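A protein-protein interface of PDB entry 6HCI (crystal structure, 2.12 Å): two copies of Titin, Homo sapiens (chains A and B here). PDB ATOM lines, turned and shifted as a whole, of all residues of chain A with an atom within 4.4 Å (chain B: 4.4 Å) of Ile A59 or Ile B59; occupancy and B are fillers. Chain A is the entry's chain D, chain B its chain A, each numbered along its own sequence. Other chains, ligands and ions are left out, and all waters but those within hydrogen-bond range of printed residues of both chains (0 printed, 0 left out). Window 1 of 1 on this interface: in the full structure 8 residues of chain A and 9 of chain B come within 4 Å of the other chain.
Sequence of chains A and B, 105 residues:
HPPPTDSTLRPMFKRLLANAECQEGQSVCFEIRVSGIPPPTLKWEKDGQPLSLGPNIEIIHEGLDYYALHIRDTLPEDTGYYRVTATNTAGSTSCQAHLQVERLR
N of His A61 sits at hydrogen-bond distance from O of Ile B59, at 2.7 Å.
N of His B61 lies within hydrogen-bond range of O of Ile A59 (2.8 Å).
Among the printed residues, merely in contact across the chains: Leu A53 with His B61, Glu A58 with Ile B60, Glu A58 with His B61, Ile A59 with Ile B59, Ile A59 with Ile B60, Ile A60 with Glu B58, Ile A60 with Ile B59, His A61 with Leu B53 and His A61 with Glu B58.
Of the printed residues of chain B, Ile A59 touches Ile B59 (3.7 Å), Ile B60 (3.4 Å) and His B61 (2.8 Å).
Of the printed residues of chain A, Ile B59 touches Ile A59, Ile A60 and His A61.
Printed residues of chain A within 4 Å of Leu B53: His A61.
Of the printed residues of chain A, Ile B60 touches Glu A58 and Ile A59.
Of the printed residues of chain A, His B61 touches Leu A53 (3.5 Å), Glu A58 (3.4 Å) and Ile A59 (2.8 Å).
Of the printed residues of chain A, Glu B58 touches Ile A60 (3.4 Å) and His A61 (3.4 Å).
The nearest printed residue of chain A that does not touch Ile B59 is Ala A68 (7.1 Å).
The nearest printed residue of chain A that does not touch Ile B60 is Ile A60 (4.2 Å).
Of the 8 printed residues of chain A, 5 touch a printed residue of chain B.
Hydrophobic or aromatic side chains of chain A within 4 Å of the printed part of chain B: Leu A53, Ile A60 and His A61.
Hydrophobic or aromatic side chains of chain B within 4 Å of the printed part of chain A: Leu B53, Ile B60 and His B61.
Among the printed residues, 11 pairs touch across the chains.
Glu A58 touches Ile B60, and with the chains exchanged Ile A60 touches Glu B58.
Glu A58 touches His B61, and with the chains exchanged His A61 touches Glu B58.
Ile A59 touches its own counterpart, Ile B59.
Ile A59 touches Ile B60, and with the chains exchanged Ile A60 touches Ile B59.
Of the 11 pairs that touch across the chains among the printed residues, 11 have their exchanged pair printed and touching as well.
O of Ile B60 sits at hydrogen-bond distance from N of Ala B68, 2.7 Å away.
N of Ile A60 sits at hydrogen-bond distance from O of Ala A68, 2.8 Å away.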
ATOM      1  N   TRP A  44     -12.455  13.533 -16.100  1.00  0.00           N
ATOM      2  CA  TRP A  44     -11.323  14.401 -16.384  1.00  0.00           C
ATOM      3  C   TRP A  44     -10.014  13.630 -16.271  1.00  0.00           C
ATOM      4  O   TRP A  44      -9.827  12.831 -15.348  1.00  0.00           O
ATOM      5  CB  TRP A  44     -11.305  15.593 -15.428  1.00  0.00           C
ATOM      6  CG  TRP A  44     -12.545  16.435 -15.481  1.00  0.00           C
ATOM      7  CD1 TRP A  44     -13.771  16.138 -14.947  1.00  0.00           C
ATOM      8  CD2 TRP A  44     -12.680  17.714 -16.111  1.00  0.00           C
ATOM      9  NE1 TRP A  44     -14.656  17.163 -15.195  1.00  0.00           N
ATOM     10  CE2 TRP A  44     -14.012  18.140 -15.911  1.00  0.00           C
ATOM     11  CE3 TRP A  44     -11.804  18.542 -16.822  1.00  0.00           C
ATOM     12  CZ2 TRP A  44     -14.489  19.355 -16.400  1.00  0.00           C
ATOM     13  CZ3 TRP A  44     -12.278  19.750 -17.305  1.00  0.00           C
ATOM     14  CH2 TRP A  44     -13.608  20.146 -17.091  1.00  0.00           C
ATOM     15  N   LEU A  51      -7.507  12.334 -13.610  1.00  0.00           N
ATOM     16  CA  LEU A  51      -7.082  13.590 -12.999  1.00  0.00           C
ATOM     17  C   LEU A  51      -7.167  13.507 -11.482  1.00  0.00           C
ATOM     18  O   LEU A  51      -8.209  13.159 -10.920  1.00  0.00           O
ATOM     19  CB  LEU A  51      -7.935  14.753 -13.510  1.00  0.00           C
ATOM     20  CG  LEU A  51      -7.680  16.107 -12.839  1.00  0.00           C
ATOM     21  CD1 LEU A  51      -6.372  16.713 -13.318  1.00  0.00           C
ATOM     22  CD2 LEU A  51      -8.834  17.071 -13.076  1.00  0.00           C
ATOM     23  N   LEU A  53      -7.450  15.484  -8.313  1.00  0.00           N
ATOM     24  CA  LEU A  53      -7.808  16.781  -7.746  1.00  0.00           C
ATOM     25  C   LEU A  53      -6.990  16.994  -6.481  1.00  0.00           C
ATOM     26  O   LEU A  53      -7.343  16.508  -5.405  1.00  0.00           O
ATOM     27  CB  LEU A  53      -9.300  16.849  -7.444  1.00  0.00           C
ATOM     28  CG  LEU A  53     -10.322  16.747  -8.575  1.00  0.00           C
ATOM     29  CD1 LEU A  53     -11.729  16.784  -8.011  1.00  0.00           C
ATOM     30  CD2 LEU A  53     -10.135  17.861  -9.576  1.00  0.00           C
ATOM     31  N   GLU A  58     -10.150  22.311  -8.287  1.00  0.00           N
ATOM     32  CA  GLU A  58     -11.563  22.048  -8.077  1.00  0.00           C
ATOM     33  C   GLU A  58     -12.287  22.087  -9.411  1.00  0.00           C
ATOM     34  O   GLU A  58     -11.863  22.763 -10.354  1.00  0.00           O
ATOM     35  CB  GLU A  58     -12.190  23.046  -7.098  1.00  0.00           C
ATOM     36  CG  GLU A  58     -12.156  24.478  -7.570  1.00  0.00           C
ATOM     37  CD  GLU A  58     -12.794  25.427  -6.579  1.00  0.00           C
ATOM     38  OE1 GLU A  58     -13.364  26.449  -7.018  1.00  0.00           O
ATOM     39  OE2 GLU A  58     -12.720  25.149  -5.361  1.00  0.00           O
ATOM     40  N   ILE A  59     -13.380  21.334  -9.483  1.00  0.00           N
ATOM     41  CA  ILE A  59     -14.225  21.279 -10.666  1.00  0.00           C
ATOM     42  C   ILE A  59     -15.597  21.784 -10.261  1.00  0.00           C
ATOM     43  O   ILE A  59     -16.194  21.267  -9.311  1.00  0.00           O
ATOM     44  CB  ILE A  59     -14.301  19.860 -11.236  1.00  0.00           C
ATOM     45  CG1 ILE A  59     -12.918  19.469 -11.748  1.00  0.00           C
ATOM     46  CG2 ILE A  59     -15.336  19.800 -12.346  1.00  0.00           C
ATOM     47  CD1 ILE A  59     -12.927  18.398 -12.752  1.00  0.00           C
ATOM     48  N   ILE A  60     -16.089  22.793 -10.972  1.00  0.00           N
ATOM     49  CA  ILE A  60     -17.321  23.489 -10.622  1.00  0.00           C
ATOM     50  C   ILE A  60     -18.367  23.226 -11.692  1.00  0.00           C
ATOM     51  O   ILE A  60     -18.090  23.360 -12.890  1.00  0.00           O
ATOM     52  CB  ILE A  60     -17.087  25.001 -10.465  1.00  0.00           C
ATOM     53  CG1 ILE A  60     -15.997  25.268  -9.423  1.00  0.00           C
ATOM     54  CG2 ILE A  60     -18.382  25.694 -10.094  1.00  0.00           C
ATOM     55  CD1 ILE A  60     -15.727  26.737  -9.196  1.00  0.00           C
ATOM     56  N   HIS A  61     -19.571  22.878 -11.261  1.00  0.00           N
ATOM     57  CA  HIS A  61     -20.720  22.741 -12.141  1.00  0.00           C
ATOM     58  C   HIS A  61     -21.695  23.869 -11.828  1.00  0.00           C
ATOM     59  O   HIS A  61     -22.141  24.007 -10.682  1.00  0.00           O
ATOM     60  CB  HIS A  61     -21.377  21.373 -11.954  1.00  0.00           C
ATOM     61  CG  HIS A  61     -22.522  21.111 -12.880  1.00  0.00           C
ATOM     62  ND1 HIS A  61     -22.692  21.787 -14.069  1.00  0.00           N
ATOM     63  CD2 HIS A  61     -23.554  20.237 -12.795  1.00  0.00           C
ATOM     64  CE1 HIS A  61     -23.781  21.346 -14.673  1.00  0.00           C
ATOM     65  NE2 HIS A  61     -24.321  20.403 -13.923  1.00  0.00           N
ATOM     66  N   ALA A  68     -16.368  24.113 -15.063  1.00  0.00           N
ATOM     67  CA  ALA A  68     -15.082  24.791 -15.049  1.00  0.00           C
ATOM     68  C   ALA A  68     -14.080  24.010 -14.217  1.00  0.00           C
ATOM     69  O   ALA A  68     -14.413  23.485 -13.151  1.00  0.00           O
ATOM     70  CB  ALA A  68     -15.201  26.219 -14.507  1.00  0.00           C
ATOM     71  N   TRP B  44     -28.422  15.118  -7.971  1.00  0.00           N
ATOM     72  CA  TRP B  44     -28.887  15.992  -6.899  1.00  0.00           C
ATOM     73  C   TRP B  44     -30.354  16.338  -7.102  1.00  0.00           C
ATOM     74  O   TRP B  44     -30.789  16.600  -8.227  1.00  0.00           O
ATOM     75  CB  TRP B  44     -28.070  17.275  -6.840  1.00  0.00           C
ATOM     76  CG  TRP B  44     -26.629  17.053  -6.628  1.00  0.00           C
ATOM     77  CD1 TRP B  44     -25.699  16.710  -7.574  1.00  0.00           C
ATOM     78  CD2 TRP B  44     -25.921  17.186  -5.396  1.00  0.00           C
ATOM     79  NE1 TRP B  44     -24.457  16.614  -6.998  1.00  0.00           N
ATOM     80  CE2 TRP B  44     -24.566  16.898  -5.661  1.00  0.00           C
ATOM     81  CE3 TRP B  44     -26.303  17.507  -4.087  1.00  0.00           C
ATOM     82  CZ2 TRP B  44     -23.590  16.926  -4.668  1.00  0.00           C
ATOM     83  CZ3 TRP B  44     -25.331  17.537  -3.100  1.00  0.00           C
ATOM     84  CH2 TRP B  44     -23.989  17.253  -3.400  1.00  0.00           C
ATOM     85  N   LEU B  53     -29.714  24.264 -11.020  1.00  0.00           N
ATOM     86  CA  LEU B  53     -28.672  25.063 -10.387  1.00  0.00           C
ATOM     87  C   LEU B  53     -28.966  26.554 -10.486  1.00  0.00           C
ATOM     88  O   LEU B  53     -28.698  27.304  -9.540  1.00  0.00           O
ATOM     89  CB  LEU B  53     -27.312  24.740 -11.003  1.00  0.00           C
ATOM     90  CG  LEU B  53     -26.847  23.298 -10.796  1.00  0.00           C
ATOM     91  CD1 LEU B  53     -25.505  23.060 -11.466  1.00  0.00           C
ATOM     92  CD2 LEU B  53     -26.772  22.991  -9.315  1.00  0.00           C
ATOM     93  N   GLU B  58     -24.130  26.195  -7.138  1.00  0.00           N
ATOM     94  CA  GLU B  58     -23.043  25.513  -7.821  1.00  0.00           C
ATOM     95  C   GLU B  58     -22.678  24.237  -7.077  1.00  0.00           C
ATOM     96  O   GLU B  58     -22.836  24.138  -5.857  1.00  0.00           O
ATOM     97  CB  GLU B  58     -21.807  26.416  -7.954  1.00  0.00           C
ATOM     98  CG  GLU B  58     -21.132  26.755  -6.637  1.00  0.00           C
ATOM     99  CD  GLU B  58     -19.969  27.715  -6.816  1.00  0.00           C
ATOM    100  OE1 GLU B  58     -19.650  28.047  -7.981  1.00  0.00           O
ATOM    101  OE2 GLU B  58     -19.385  28.150  -5.797  1.00  0.00           O
ATOM    102  N   ILE B  59     -22.204  23.251  -7.835  1.00  0.00           N
ATOM    103  CA  ILE B  59     -21.676  22.006  -7.292  1.00  0.00           C
ATOM    104  C   ILE B  59     -20.170  22.017  -7.485  1.00  0.00           C
ATOM    105  O   ILE B  59     -19.685  22.284  -8.592  1.00  0.00           O
ATOM    106  CB  ILE B  59     -22.294  20.775  -7.974  1.00  0.00           C
ATOM    107  CG1 ILE B  59     -23.820  20.901  -8.047  1.00  0.00           C
ATOM    108  CG2 ILE B  59     -21.845  19.495  -7.262  1.00  0.00           C
ATOM    109  CD1 ILE B  59     -24.539  20.422  -6.816  1.00  0.00           C
ATOM    110  N   ILE B  60     -19.432  21.725  -6.417  1.00  0.00           N
ATOM    111  CA  ILE B  60     -17.977  21.737  -6.442  1.00  0.00           C
ATOM    112  C   ILE B  60     -17.460  20.341  -6.120  1.00  0.00           C
ATOM    113  O   ILE B  60     -17.916  19.704  -5.163  1.00  0.00           O
ATOM    114  CB  ILE B  60     -17.410  22.778  -5.464  1.00  0.00           C
ATOM    115  CG1 ILE B  60     -17.904  24.169  -5.858  1.00  0.00           C
ATOM    116  CG2 ILE B  60     -15.894  22.750  -5.479  1.00  0.00           C
ATOM    117  CD1 ILE B  60     -17.727  25.200  -4.771  1.00  0.00           C
ATOM    118  N   HIS B  61     -16.525  19.867  -6.930  1.00  0.00           N
ATOM    119  CA  HIS B  61     -15.835  18.604  -6.717  1.00  0.00           C
ATOM    120  C   HIS B  61     -14.393  18.933  -6.357  1.00  0.00           C
ATOM    121  O   HIS B  61     -13.710  19.631  -7.110  1.00  0.00           O
ATOM    122  CB  HIS B  61     -15.913  17.738  -7.975  1.00  0.00           C
ATOM    123  CG  HIS B  61     -15.353  16.359  -7.810  1.00  0.00           C
ATOM    124  ND1 HIS B  61     -15.280  15.722  -6.591  1.00  0.00           N
ATOM    125  CD2 HIS B  61     -14.850  15.491  -8.721  1.00  0.00           C
ATOM    126  CE1 HIS B  61     -14.750  14.522  -6.755  1.00  0.00           C
ATOM    127  NE2 HIS B  61     -14.481  14.358  -8.038  1.00  0.00           N
ATOM    128  N   ALA B  68     -19.185  19.605  -2.744  1.00  0.00           N
ATOM    129  CA  ALA B  68     -19.854  20.647  -1.981  1.00  0.00           C
ATOM    130  C   ALA B  68     -20.978  21.252  -2.804  1.00  0.00           C
ATOM    131  O   ALA B  68     -20.855  21.417  -4.020  1.00  0.00           O
ATOM    132  CB  ALA B  68     -18.883  21.753  -1.541  1.00  0.00           C
ATOM    133  N   LEU B  69     -22.089  21.542  -2.139  1.00  0.00           N
ATOM    134  CA  LEU B  69     -23.200  22.275  -2.726  1.00  0.00           C
ATOM    135  C   LEU B  69     -23.221  23.656  -2.087  1.00  0.00           C
ATOM    136  O   LEU B  69     -23.423  23.781  -0.875  1.00  0.00           O
ATOM    137  CB  LEU B  69     -24.526  21.549  -2.503  1.00  0.00           C
ATOM    138  CG  LEU B  69     -25.736  22.005  -3.326  1.00  0.00           C
ATOM    139  CD1 LEU B  69     -26.738  20.873  -3.441  1.00  0.00           C
ATOM    140  CD2 LEU B  69     -26.401  23.225  -2.710  1.00  0.00           C
